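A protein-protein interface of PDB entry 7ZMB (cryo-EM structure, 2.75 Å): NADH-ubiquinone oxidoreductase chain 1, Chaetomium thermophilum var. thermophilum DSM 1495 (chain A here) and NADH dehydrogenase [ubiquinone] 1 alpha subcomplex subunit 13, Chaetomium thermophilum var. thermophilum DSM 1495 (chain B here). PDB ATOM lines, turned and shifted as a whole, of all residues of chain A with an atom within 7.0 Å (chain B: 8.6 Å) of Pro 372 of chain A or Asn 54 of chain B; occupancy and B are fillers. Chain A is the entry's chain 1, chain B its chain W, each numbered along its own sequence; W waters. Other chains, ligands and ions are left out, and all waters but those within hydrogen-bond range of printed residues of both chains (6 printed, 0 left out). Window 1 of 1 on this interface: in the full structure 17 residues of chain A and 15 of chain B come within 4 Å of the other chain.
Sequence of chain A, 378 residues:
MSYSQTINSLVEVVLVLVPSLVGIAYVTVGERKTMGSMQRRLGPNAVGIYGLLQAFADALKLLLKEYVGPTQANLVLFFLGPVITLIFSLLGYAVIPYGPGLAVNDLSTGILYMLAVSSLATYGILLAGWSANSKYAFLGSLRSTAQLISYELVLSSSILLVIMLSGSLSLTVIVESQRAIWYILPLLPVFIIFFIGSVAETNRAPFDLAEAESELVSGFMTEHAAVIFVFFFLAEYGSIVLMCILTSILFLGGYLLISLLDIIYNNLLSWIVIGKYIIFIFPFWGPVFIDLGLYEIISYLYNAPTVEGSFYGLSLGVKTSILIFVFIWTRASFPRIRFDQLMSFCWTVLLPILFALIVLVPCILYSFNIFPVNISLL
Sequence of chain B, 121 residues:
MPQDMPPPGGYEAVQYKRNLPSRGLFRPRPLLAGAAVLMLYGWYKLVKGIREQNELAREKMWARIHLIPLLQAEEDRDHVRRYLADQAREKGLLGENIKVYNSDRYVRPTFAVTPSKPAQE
Printed residues of chain A that touch a printed residue of chain B: Leu 165, Tyr 183, Ile 370, Phe 371, Pro 372, Val 373, Ile 375 and Leu 377.
Hydrophobic or aromatic side chains of chain B within 4 Å of the printed part of chain A: Leu 46, Val 47, Ile 50, Ala 57 and Met 61.
Along chain B the printed residues that touch a printed residue of chain A span positions 46 to 61.
Among the printed residues, no Asp or Glu carboxylate lies within 4 Å of a Lys or Arg side-chain nitrogen of the other chain.
Pro 372 of chain A touches three residues of chain B.
Asn 54 of chain B touches just these residues of chain A: Phe 371 (3.0 Å), Pro 372 (3.9 Å) and Val 373 (3.3 Å).
Val 373 of chain A touches two residues of chain B.
Of the printed residues of chain A, Lys 60 of chain B touches Leu 377 (3.5 Å).
Printed residues of chain A within 4 Å of Met 61 of chain B: Ile 375.
Of the printed residues of chain A, Val 47 of chain B touches Ile 370 (3.6 Å).
Gly 167 of chain A touches none of the printed residues of chain B.
Ser 177 of chain A touches none of the printed residues of chain B.
The nearest printed residue of chain B that does not touch Pro 372 of chain A is Ala 57 of chain B (7.6 Å).
The nearest residue of chain A that does not touch Asn 54 of chain B is Asn 369 of chain A (4.6 Å).
O of Leu 365 of chain A is in hydrogen-bond range of N of Ile 370 of chain A, 2.7 Å away.
The side-chain amide oxygen of Asn 374 of chain A lies close to the backbone carbonyl oxygen of Pro 372 of chain A.
O of Ile 50 of chain B lies close to OD1 of Asn 54 of chain B, 3.4 Å away.
Water W1 lies within hydrogen-bond range of the backbone carbonyl oxygen of Leu 165 of chain A and the side-chain amide nitrogen of Gln 53 of chain B.
Water W5 lies within hydrogen-bond range of O of Asn 369 of chain A and ND2 of Asn 54 of chain B.
Water W4 bridges O of Leu 377 of chain A and NZ of Lys 60 of chain B.
Water W2 bridges OE1 of Gln 53 of chain B (2.9 Å) and O of Ser 177 of chain A (3.4 Å).
Water W3 bridges NE2 of Gln 53 of chain B and O of Val 373 of chain A.
Water W6 lies within hydrogen-bond range of O of Phe 371 of chain A and ND2 of Asn 54 of chain B.
CD2 of Leu 46 of chain B touches CD1 of Leu 165 of chain A, 3.6 Å away.
CD1 of Leu 46 of chain B touches CE1 of Tyr 183 of chain A (3.8 Å).
CD1 of Ile 370 of chain A touches CG2 of Val 47 of chain B, 3.6 Å away.
O of Ile 370 of chain A touches CD1 of Ile 50 of chain B, at 3.3 Å.
Pro 372 of chain A touches Ile 50 of chain B.
Gln 53 of chain B touches Pro 372 of chain A (NE2 to CB, 3.4 Å).
CA of Pro 372 of chain A touches OD1 of Asn 54 of chain B, at 3.9 Å.
Val 373 of chain A touches Ala 57 of chain B (CG2 to CB, 3.5 Å).
CE of Met 61 of chain B touches CD1 of Ile 375 of chain A, at 3.99 Å.
Leu 377 of chain A touches Lys 60 of chain B.
The backbone carbonyl oxygen (O) of Phe 371 of chain A is in hydrogen-bond range of the side-chain amide nitrogen (ND2) of Asn 54 of chain B, 3.0 Å away.
OD1 of Asn 54 of chain B lies within hydrogen-bond range of N of Val 373 of chain A (3.3 Å).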
ATOM      1  N   ILE A 163      16.248   5.122   9.551  1.00  0.00           N
ATOM      2  CA  ILE A 163      16.117   6.375   8.760  1.00  0.00           C
ATOM      3  C   ILE A 163      14.872   6.301   7.869  1.00  0.00           C
ATOM      4  O   ILE A 163      14.243   7.335   7.665  1.00  0.00           O
ATOM      5  CB  ILE A 163      17.411   6.696   7.990  1.00  0.00           C
ATOM      6  CG1 ILE A 163      18.663   6.264   8.759  1.00  0.00           C
ATOM      7  CG2 ILE A 163      17.451   8.166   7.608  1.00  0.00           C
ATOM      8  CD1 ILE A 163      18.853   6.949  10.094  1.00  0.00           C
ATOM      9  N   MET A 164      14.524   5.121   7.369  1.00  0.00           N
ATOM     10  CA  MET A 164      13.281   4.995   6.574  1.00  0.00           C
ATOM     11  C   MET A 164      12.076   5.405   7.431  1.00  0.00           C
ATOM     12  O   MET A 164      11.216   6.111   6.906  1.00  0.00           O
ATOM     13  CB  MET A 164      13.127   3.586   6.011  1.00  0.00           C
ATOM     14  CG  MET A 164      14.185   3.237   4.986  1.00  0.00           C
ATOM     15  SD  MET A 164      14.222   1.469   4.613  1.00  0.00           S
ATOM     16  CE  MET A 164      15.432   1.427   3.291  1.00  0.00           C
ATOM     17  N   LEU A 165      12.003   4.979   8.697  1.00  0.00           N
ATOM     18  CA  LEU A 165      10.901   5.464   9.573  1.00  0.00           C
ATOM     19  C   LEU A 165      11.044   6.948   9.933  1.00  0.00           C
ATOM     20  O   LEU A 165      10.038   7.645   9.835  1.00  0.00           O
ATOM     21  CB  LEU A 165      10.838   4.620  10.847  1.00  0.00           C
ATOM     22  CG  LEU A 165      10.650   3.116  10.671  1.00  0.00           C
ATOM     23  CD1 LEU A 165      10.209   2.496  11.983  1.00  0.00           C
ATOM     24  CD2 LEU A 165       9.637   2.814   9.580  1.00  0.00           C
ATOM     25  N   SER A 166      12.221   7.402  10.376  1.00  0.00           N
ATOM     26  CA  SER A 166      12.399   8.809  10.841  1.00  0.00           C
ATOM     27  C   SER A 166      12.408   9.805   9.684  1.00  0.00           C
ATOM     28  O   SER A 166      11.766  10.852   9.817  1.00  0.00           O
ATOM     29  CB  SER A 166      13.623   8.943  11.693  1.00  0.00           C
ATOM     30  OG  SER A 166      14.803   8.745  10.930  1.00  0.00           O
ATOM     31  N   GLY A 167      13.144   9.488   8.616  1.00  0.00           N
ATOM     32  CA  GLY A 167      13.264  10.356   7.434  1.00  0.00           C
ATOM     33  C   GLY A 167      14.260  11.468   7.665  1.00  0.00           C
ATOM     34  O   GLY A 167      14.305  12.386   6.833  1.00  0.00           O
ATOM     35  N   SER A 168      15.059  11.388   8.733  1.00  0.00           N
ATOM     36  CA  SER A 168      15.892  12.575   9.041  1.00  0.00           C
ATOM     37  C   SER A 168      17.405  12.432   8.989  1.00  0.00           C
ATOM     38  O   SER A 168      17.993  13.314   8.321  1.00  0.00           O
ATOM     39  CB  SER A 168      15.469  13.230  10.298  1.00  0.00           C
ATOM     40  OG  SER A 168      16.272  14.367  10.549  1.00  0.00           O
ATOM     41  N   SER A 177      10.548  11.544  16.734  1.00  0.00           N
ATOM     42  CA  SER A 177       9.649  10.648  15.960  1.00  0.00           C
ATOM     43  C   SER A 177       9.136   9.513  16.855  1.00  0.00           C
ATOM     44  O   SER A 177       7.999   9.086  16.650  1.00  0.00           O
ATOM     45  CB  SER A 177      10.342  10.149  14.714  1.00  0.00           C
ATOM     46  OG  SER A 177      10.747  11.226  13.888  1.00  0.00           O
ATOM     47  N   TYR A 183      11.062   2.705  18.624  1.00  0.00           N
ATOM     48  CA  TYR A 183      11.349   1.921  17.389  1.00  0.00           C
ATOM     49  C   TYR A 183      11.721   0.471  17.716  1.00  0.00           C
ATOM     50  O   TYR A 183      11.902  -0.288  16.787  1.00  0.00           O
ATOM     51  CB  TYR A 183      12.386   2.609  16.499  1.00  0.00           C
ATOM     52  CG  TYR A 183      11.913   3.827  15.751  1.00  0.00           C
ATOM     53  CD1 TYR A 183      10.567   4.071  15.549  1.00  0.00           C
ATOM     54  CD2 TYR A 183      12.823   4.728  15.224  1.00  0.00           C
ATOM     55  CE1 TYR A 183      10.137   5.188  14.854  1.00  0.00           C
ATOM     56  CE2 TYR A 183      12.410   5.848  14.523  1.00  0.00           C
ATOM     57  CZ  TYR A 183      11.061   6.076  14.338  1.00  0.00           C
ATOM     58  OH  TYR A 183      10.638   7.169  13.647  1.00  0.00           O
ATOM     59  N   LEU A 365       5.532   0.821   4.232  1.00  0.00           N
ATOM     60  CA  LEU A 365       5.327   2.289   4.376  1.00  0.00           C
ATOM     61  C   LEU A 365       4.452   2.858   3.250  1.00  0.00           C
ATOM     62  O   LEU A 365       3.473   3.536   3.571  1.00  0.00           O
ATOM     63  CB  LEU A 365       6.692   2.972   4.420  1.00  0.00           C
ATOM     64  CG  LEU A 365       7.601   2.596   5.590  1.00  0.00           C
ATOM     65  CD1 LEU A 365       8.928   3.333   5.505  1.00  0.00           C
ATOM     66  CD2 LEU A 365       6.927   2.873   6.920  1.00  0.00           C
ATOM     67  N   ASN A 369       0.513   4.294   3.482  1.00  0.00           N
ATOM     68  CA  ASN A 369       0.623   5.767   3.324  1.00  0.00           C
ATOM     69  C   ASN A 369       1.414   6.369   4.486  1.00  0.00           C
ATOM     70  O   ASN A 369       1.038   7.453   4.946  1.00  0.00           O
ATOM     71  CB  ASN A 369      -0.740   6.444   3.175  1.00  0.00           C
ATOM     72  CG  ASN A 369      -0.656   7.777   2.470  1.00  0.00           C
ATOM     73  OD1 ASN A 369      -1.374   8.711   2.814  1.00  0.00           O
ATOM     74  ND2 ASN A 369       0.235   7.877   1.498  1.00  0.00           N
ATOM     75  N   ILE A 370       2.458   5.684   4.955  1.00  0.00           N
ATOM     76  CA  ILE A 370       3.204   6.202   6.134  1.00  0.00           C
ATOM     77  C   ILE A 370       4.661   6.536   5.813  1.00  0.00           C
ATOM     78  O   ILE A 370       5.511   6.270   6.673  1.00  0.00           O
ATOM     79  CB  ILE A 370       3.016   5.327   7.394  1.00  0.00           C
ATOM     80  CG1 ILE A 370       3.334   3.854   7.135  1.00  0.00           C
ATOM     81  CG2 ILE A 370       1.614   5.508   7.949  1.00  0.00           C
ATOM     82  CD1 ILE A 370       3.633   3.077   8.388  1.00  0.00           C
ATOM     83  N   PHE A 371       4.945   7.089   4.636  1.00  0.00           N
ATOM     84  CA  PHE A 371       6.324   7.584   4.383  1.00  0.00           C
ATOM     85  C   PHE A 371       6.421   8.904   5.151  1.00  0.00           C
ATOM     86  O   PHE A 371       5.540   9.763   4.992  1.00  0.00           O
ATOM     87  CB  PHE A 371       6.613   7.853   2.904  1.00  0.00           C
ATOM     88  CG  PHE A 371       7.006   6.673   2.055  1.00  0.00           C
ATOM     89  CD1 PHE A 371       7.859   5.694   2.537  1.00  0.00           C
ATOM     90  CD2 PHE A 371       6.566   6.571   0.746  1.00  0.00           C
ATOM     91  CE1 PHE A 371       8.235   4.627   1.739  1.00  0.00           C
ATOM     92  CE2 PHE A 371       6.944   5.504  -0.051  1.00  0.00           C
ATOM     93  CZ  PHE A 371       7.777   4.532   0.448  1.00  0.00           C
ATOM     94  N   PRO A 372       7.440   9.099   6.003  1.00  0.00           N
ATOM     95  CA  PRO A 372       7.588  10.356   6.716  1.00  0.00           C
ATOM     96  C   PRO A 372       7.947  11.540   5.811  1.00  0.00           C
ATOM     97  O   PRO A 372       8.710  11.361   4.898  1.00  0.00           O
ATOM     98  CB  PRO A 372       8.737  10.045   7.683  1.00  0.00           C
ATOM     99  CG  PRO A 372       9.543   8.996   6.966  1.00  0.00           C
ATOM    100  CD  PRO A 372       8.496   8.131   6.304  1.00  0.00           C
ATOM    101  N   VAL A 373       7.392  12.715   6.095  1.00  0.00           N
ATOM    102  CA  VAL A 373       7.808  13.938   5.354  1.00  0.00           C
ATOM    103  C   VAL A 373       9.282  14.162   5.703  1.00  0.00           C
ATOM    104  O   VAL A 373       9.659  13.919   6.859  1.00  0.00           O
ATOM    105  CB  VAL A 373       6.918  15.160   5.645  1.00  0.00           C
ATOM    106  CG1 VAL A 373       5.529  15.019   5.053  1.00  0.00           C
ATOM    107  CG2 VAL A 373       6.836  15.467   7.128  1.00  0.00           C
ATOM    108  N   ASN A 374      10.091  14.572   4.736  1.00  0.00           N
ATOM    109  CA  ASN A 374      11.556  14.659   4.976  1.00  0.00           C
ATOM    110  C   ASN A 374      11.943  16.121   5.198  1.00  0.00           C
ATOM    111  O   ASN A 374      13.135  16.430   5.159  1.00  0.00           O
ATOM    112  CB  ASN A 374      12.288  13.907   3.863  1.00  0.00           C
ATOM    113  CG  ASN A 374      11.854  12.463   3.746  1.00  0.00           C
ATOM    114  OD1 ASN A 374      11.158  12.089   2.811  1.00  0.00           O
ATOM    115  ND2 ASN A 374      12.250  11.641   4.699  1.00  0.00           N
ATOM    116  N   ILE A 375      10.953  16.966   5.450  1.00  0.00           N
ATOM    117  CA  ILE A 375      11.186  18.406   5.747  1.00  0.00           C
ATOM    118  C   ILE A 375      11.613  18.522   7.209  1.00  0.00           C
ATOM    119  O   ILE A 375      11.552  17.511   7.925  1.00  0.00           O
ATOM    120  CB  ILE A 375       9.882  19.188   5.485  1.00  0.00           C
ATOM    121  CG1 ILE A 375       8.789  18.845   6.498  1.00  0.00           C
ATOM    122  CG2 ILE A 375       9.409  18.989   4.053  1.00  0.00           C
ATOM    123  CD1 ILE A 375       7.580  19.744   6.414  1.00  0.00           C
ATOM    124  N   LEU A 377      10.675  19.318  10.805  1.00  0.00           N
ATOM    125  CA  LEU A 377       9.398  19.425  11.556  1.00  0.00           C
ATOM    126  C   LEU A 377       9.688  19.189  13.034  1.00  0.00           C
ATOM    127  O   LEU A 377       9.482  20.116  13.835  1.00  0.00           O
ATOM    128  CB  LEU A 377       8.413  18.389  11.007  1.00  0.00           C
ATOM    129  CG  LEU A 377       7.053  18.323  11.697  1.00  0.00           C
ATOM    130  CD1 LEU A 377       6.198  19.524  11.328  1.00  0.00           C
ATOM    131  CD2 LEU A 377       6.341  17.029  11.340  1.00  0.00           C
ATOM    132  N   LEU B  46       2.812   3.210  14.902  1.00  0.00           N
ATOM    133  CA  LEU B  46       3.629   3.913  13.930  1.00  0.00           C
ATOM    134  C   LEU B  46       2.771   4.486  12.809  1.00  0.00           C
ATOM    135  O   LEU B  46       3.024   5.598  12.335  1.00  0.00           O
ATOM    136  CB  LEU B  46       4.696   2.974  13.374  1.00  0.00           C
ATOM    137  CG  LEU B  46       5.787   3.679  12.565  1.00  0.00           C
ATOM    138  CD1 LEU B  46       6.685   4.504  13.493  1.00  0.00           C
ATOM    139  CD2 LEU B  46       6.589   2.711  11.728  1.00  0.00           C
ATOM    140  N   VAL B  47       1.754   3.741  12.368  1.00  0.00           N
ATOM    141  CA  VAL B  47       0.842   4.246  11.347  1.00  0.00           C
ATOM    142  C   VAL B  47       0.098   5.473  11.858  1.00  0.00           C
ATOM    143  O   VAL B  47      -0.044   6.466  11.142  1.00  0.00           O
ATOM    144  CB  VAL B  47      -0.128   3.136  10.895  1.00  0.00           C
ATOM    145  CG1 VAL B  47      -1.358   3.726  10.234  1.00  0.00           C
ATOM    146  CG2 VAL B  47       0.557   2.187   9.951  1.00  0.00           C
ATOM    147  N   LYS B  48      -0.377   5.430  13.107  1.00  0.00           N
ATOM    148  CA  LYS B  48      -0.999   6.609  13.707  1.00  0.00           C
ATOM    149  C   LYS B  48      -0.027   7.777  13.790  1.00  0.00           C
ATOM    150  O   LYS B  48      -0.384   8.916  13.476  1.00  0.00           O
ATOM    151  CB  LYS B  48      -1.526   6.273  15.103  1.00  0.00           C
ATOM    152  CG  LYS B  48      -2.586   5.184  15.188  1.00  0.00           C
ATOM    153  CD  LYS B  48      -3.931   5.624  14.628  1.00  0.00           C
ATOM    154  CE  LYS B  48      -4.122   5.251  13.170  1.00  0.00           C
ATOM    155  NZ  LYS B  48      -5.487   5.603  12.691  1.00  0.00           N
ATOM    156  N   GLY B  49       1.202   7.525  14.243  1.00  0.00           N
ATOM    157  CA  GLY B  49       2.187   8.603  14.434  1.00  0.00           C
ATOM    158  C   GLY B  49       2.537   9.329  13.157  1.00  0.00           C
ATOM    159  O   GLY B  49       2.538  10.566  13.167  1.00  0.00           O
ATOM    160  N   ILE B  50       2.924   8.576  12.128  1.00  0.00           N
ATOM    161  CA  ILE B  50       3.362   9.184  10.843  1.00  0.00           C
ATOM    162  C   ILE B  50       2.180   9.868  10.162  1.00  0.00           C
ATOM    163  O   ILE B  50       2.374  10.942   9.575  1.00  0.00           O
ATOM    164  CB  ILE B  50       4.087   8.156   9.957  1.00  0.00           C
ATOM    165  CG1 ILE B  50       5.229   7.483  10.721  1.00  0.00           C
ATOM    166  CG2 ILE B  50       4.582   8.806   8.676  1.00  0.00           C
ATOM    167  CD1 ILE B  50       5.976   6.438   9.933  1.00  0.00           C
ATOM    168  N   ARG B  51       0.993   9.279  10.263  1.00  0.00           N
ATOM    169  CA  ARG B  51      -0.182   9.952   9.672  1.00  0.00           C
ATOM    170  C   ARG B  51      -0.382  11.313  10.350  1.00  0.00           C
ATOM    171  O   ARG B  51      -0.618  12.287   9.622  1.00  0.00           O
ATOM    172  CB  ARG B  51      -1.382   9.009   9.647  1.00  0.00           C
ATOM    173  CG  ARG B  51      -1.347   8.022   8.489  1.00  0.00           C
ATOM    174  CD  ARG B  51      -2.513   7.059   8.508  1.00  0.00           C
ATOM    175  NE  ARG B  51      -2.481   6.055   7.456  1.00  0.00           N
ATOM    176  CZ  ARG B  51      -3.444   5.166   7.252  1.00  0.00           C
ATOM    177  NH1 ARG B  51      -3.337   4.281   6.275  1.00  0.00           N
ATOM    178  NH2 ARG B  51      -4.514   5.167   8.025  1.00  0.00           N
ATOM    179  N   GLU B  52      -0.237  11.385  11.675  1.00  0.00           N
ATOM    180  CA  GLU B  52      -0.382  12.660  12.427  1.00  0.00           C
ATOM    181  C   GLU B  52       0.745  13.634  12.082  1.00  0.00           C
ATOM    182  O   GLU B  52       0.447  14.822  11.933  1.00  0.00           O
ATOM    183  CB  GLU B  52      -0.446  12.388  13.929  1.00  0.00           C
ATOM    184  CG  GLU B  52      -1.270  13.413  14.679  1.00  0.00           C
ATOM    185  CD  GLU B  52      -0.838  13.674  16.107  1.00  0.00           C
ATOM    186  OE1 GLU B  52       0.379  13.684  16.350  1.00  0.00           O
ATOM    187  OE2 GLU B  52      -1.721  13.862  16.967  1.00  0.00           O
ATOM    188  N   GLN B  53       1.986  13.146  11.972  1.00  0.00           N
ATOM    189  CA  GLN B  53       3.160  14.020  11.693  1.00  0.00           C
ATOM    190  C   GLN B  53       3.057  14.621  10.287  1.00  0.00           C
ATOM    191  O   GLN B  53       3.475  15.764  10.117  1.00  0.00           O
ATOM    192  CB  GLN B  53       4.493  13.355  12.039  1.00  0.00           C
ATOM    193  CG  GLN B  53       5.049  12.457  10.948  1.00  0.00           C
ATOM    194  CD  GLN B  53       6.412  11.945  11.337  1.00  0.00           C
ATOM    195  OE1 GLN B  53       6.808  12.000  12.497  1.00  0.00           O
ATOM    196  NE2 GLN B  53       7.145  11.453  10.356  1.00  0.00           N
ATOM    197  N   ASN B  54       2.540  13.866   9.325  1.00  0.00           N
ATOM    198  CA  ASN B  54       2.372  14.387   7.949  1.00  0.00           C
ATOM    199  C   ASN B  54       1.308  15.480   7.990  1.00  0.00           C
ATOM    200  O   ASN B  54       1.482  16.466   7.266  1.00  0.00           O
ATOM    201  CB  ASN B  54       2.140  13.269   6.922  1.00  0.00           C
ATOM    202  CG  ASN B  54       3.347  12.381   6.706  1.00  0.00           C
ATOM    203  OD1 ASN B  54       4.386  12.560   7.338  1.00  0.00           O
ATOM    204  ND2 ASN B  54       3.220  11.416   5.813  1.00  0.00           N
ATOM    205  N   GLU B  55       0.243  15.292   8.777  1.00  0.00           N
ATOM    206  CA  GLU B  55      -0.779  16.348   8.978  1.00  0.00           C
ATOM    207  C   GLU B  55      -0.185  17.551   9.719  1.00  0.00           C
ATOM    208  O   GLU B  55      -0.549  18.682   9.375  1.00  0.00           O
ATOM    209  CB  GLU B  55      -1.993  15.735   9.670  1.00  0.00           C
ATOM    210  CG  GLU B  55      -2.762  14.817   8.750  1.00  0.00           C
ATOM    211  CD  GLU B  55      -2.834  15.365   7.337  1.00  0.00           C
ATOM    212  OE1 GLU B  55      -2.374  14.672   6.410  1.00  0.00           O
ATOM    213  OE2 GLU B  55      -3.356  16.485   7.170  1.00  0.00           O
ATOM    214  N   LEU B  56       0.679  17.315  10.705  1.00  0.00           N
ATOM    215  CA  LEU B  56       1.364  18.410  11.434  1.00  0.00           C
ATOM    216  C   LEU B  56       2.237  19.163  10.436  1.00  0.00           C
ATOM    217  O   LEU B  56       2.302  20.394  10.533  1.00  0.00           O
ATOM    218  CB  LEU B  56       2.209  17.795  12.553  1.00  0.00           C
ATOM    219  CG  LEU B  56       1.452  17.380  13.809  1.00  0.00           C
ATOM    220  CD1 LEU B  56       2.425  16.890  14.867  1.00  0.00           C
ATOM    221  CD2 LEU B  56       0.628  18.536  14.344  1.00  0.00           C
ATOM    222  N   ALA B  57       2.877  18.433   9.520  1.00  0.00           N
ATOM    223  CA  ALA B  57       3.710  19.046   8.463  1.00  0.00           C
ATOM    224  C   ALA B  57       2.861  19.910   7.522  1.00  0.00           C
ATOM    225  O   ALA B  57       3.355  20.966   7.121  1.00  0.00           O
ATOM    226  CB  ALA B  57       4.469  17.971   7.736  1.00  0.00           C
ATOM    227  N   ARG B  58       1.633  19.481   7.203  1.00  0.00           N
ATOM    228  CA  ARG B  58       0.729  20.257   6.310  1.00  0.00           C
ATOM    229  C   ARG B  58       0.407  21.619   6.936  1.00  0.00           C
ATOM    230  O   ARG B  58       0.417  22.612   6.201  1.00  0.00           O
ATOM    231  CB  ARG B  58      -0.564  19.480   6.064  1.00  0.00           C
ATOM    232  CG  ARG B  58      -1.508  20.125   5.061  1.00  0.00           C
ATOM    233  CD  ARG B  58      -2.830  19.390   4.984  1.00  0.00           C
ATOM    234  NE  ARG B  58      -2.644  17.952   4.868  1.00  0.00           N
ATOM    235  CZ  ARG B  58      -2.451  17.302   3.729  1.00  0.00           C
ATOM    236  NH1 ARG B  58      -2.290  15.991   3.742  1.00  0.00           N
ATOM    237  NH2 ARG B  58      -2.420  17.957   2.583  1.00  0.00           N
ATOM    238  N   GLU B  59       0.139  21.647   8.243  1.00  0.00           N
ATOM    239  CA  GLU B  59      -0.187  22.907   8.963  1.00  0.00           C
ATOM    240  C   GLU B  59       1.021  23.846   8.986  1.00  0.00           C
ATOM    241  O   GLU B  59       0.823  25.053   8.756  1.00  0.00           O
ATOM    242  CB  GLU B  59      -0.728  22.555  10.346  1.00  0.00           C
ATOM    243  CG  GLU B  59      -0.976  23.737  11.256  1.00  0.00           C
ATOM    244  CD  GLU B  59      -1.196  23.295  12.690  1.00  0.00           C
ATOM    245  OE1 GLU B  59      -1.686  24.105  13.492  1.00  0.00           O
ATOM    246  OE2 GLU B  59      -0.871  22.135  12.997  1.00  0.00           O
ATOM    247  N   LYS B  60       2.222  23.313   9.224  1.00  0.00           N
ATOM    248  CA  LYS B  60       3.452  24.155   9.302  1.00  0.00           C
ATOM    249  C   LYS B  60       3.710  24.798   7.939  1.00  0.00           C
ATOM    250  O   LYS B  60       4.113  25.962   7.911  1.00  0.00           O
ATOM    251  CB  LYS B  60       4.655  23.327   9.759  1.00  0.00           C
ATOM    252  CG  LYS B  60       5.983  24.061   9.834  1.00  0.00           C
ATOM    253  CD  LYS B  60       7.121  23.132  10.161  1.00  0.00           C
ATOM    254  CE  LYS B  60       8.318  23.842  10.747  1.00  0.00           C
ATOM    255  NZ  LYS B  60       9.187  22.898  11.484  1.00  0.00           N
ATOM    256  N   MET B  61       3.445  24.069   6.857  1.00  0.00           N
ATOM    257  CA  MET B  61       3.694  24.593   5.491  1.00  0.00           C
ATOM    258  C   MET B  61       2.664  25.666   5.118  1.00  0.00           C
ATOM    259  O   MET B  61       3.083  26.690   4.560  1.00  0.00           O
ATOM    260  CB  MET B  61       3.703  23.460   4.464  1.00  0.00           C
ATOM    261  CG  MET B  61       4.853  22.488   4.625  1.00  0.00           C
ATOM    262  SD  MET B  61       6.455  23.167   4.129  1.00  0.00           S
ATOM    263  CE  MET B  61       7.132  23.649   5.717  1.00  0.00           C
HETATM  264  O   HOH W   1       8.566   9.212  11.132  1.00  0.00           O
HETATM  265  O   HOH W   2       6.555   9.359  13.588  1.00  0.00           O
HETATM  266  O   HOH W   3       7.965  14.158   9.781  1.00  0.00           O
HETATM  267  O   HOH W   4      11.323  22.230  13.609  1.00  0.00           O
HETATM  268  O   HOH W   5       0.370  10.072   5.081  1.00  0.00           O
HETATM  269  O   HOH W   6       3.543   9.611   2.855  1.00  0.00           O
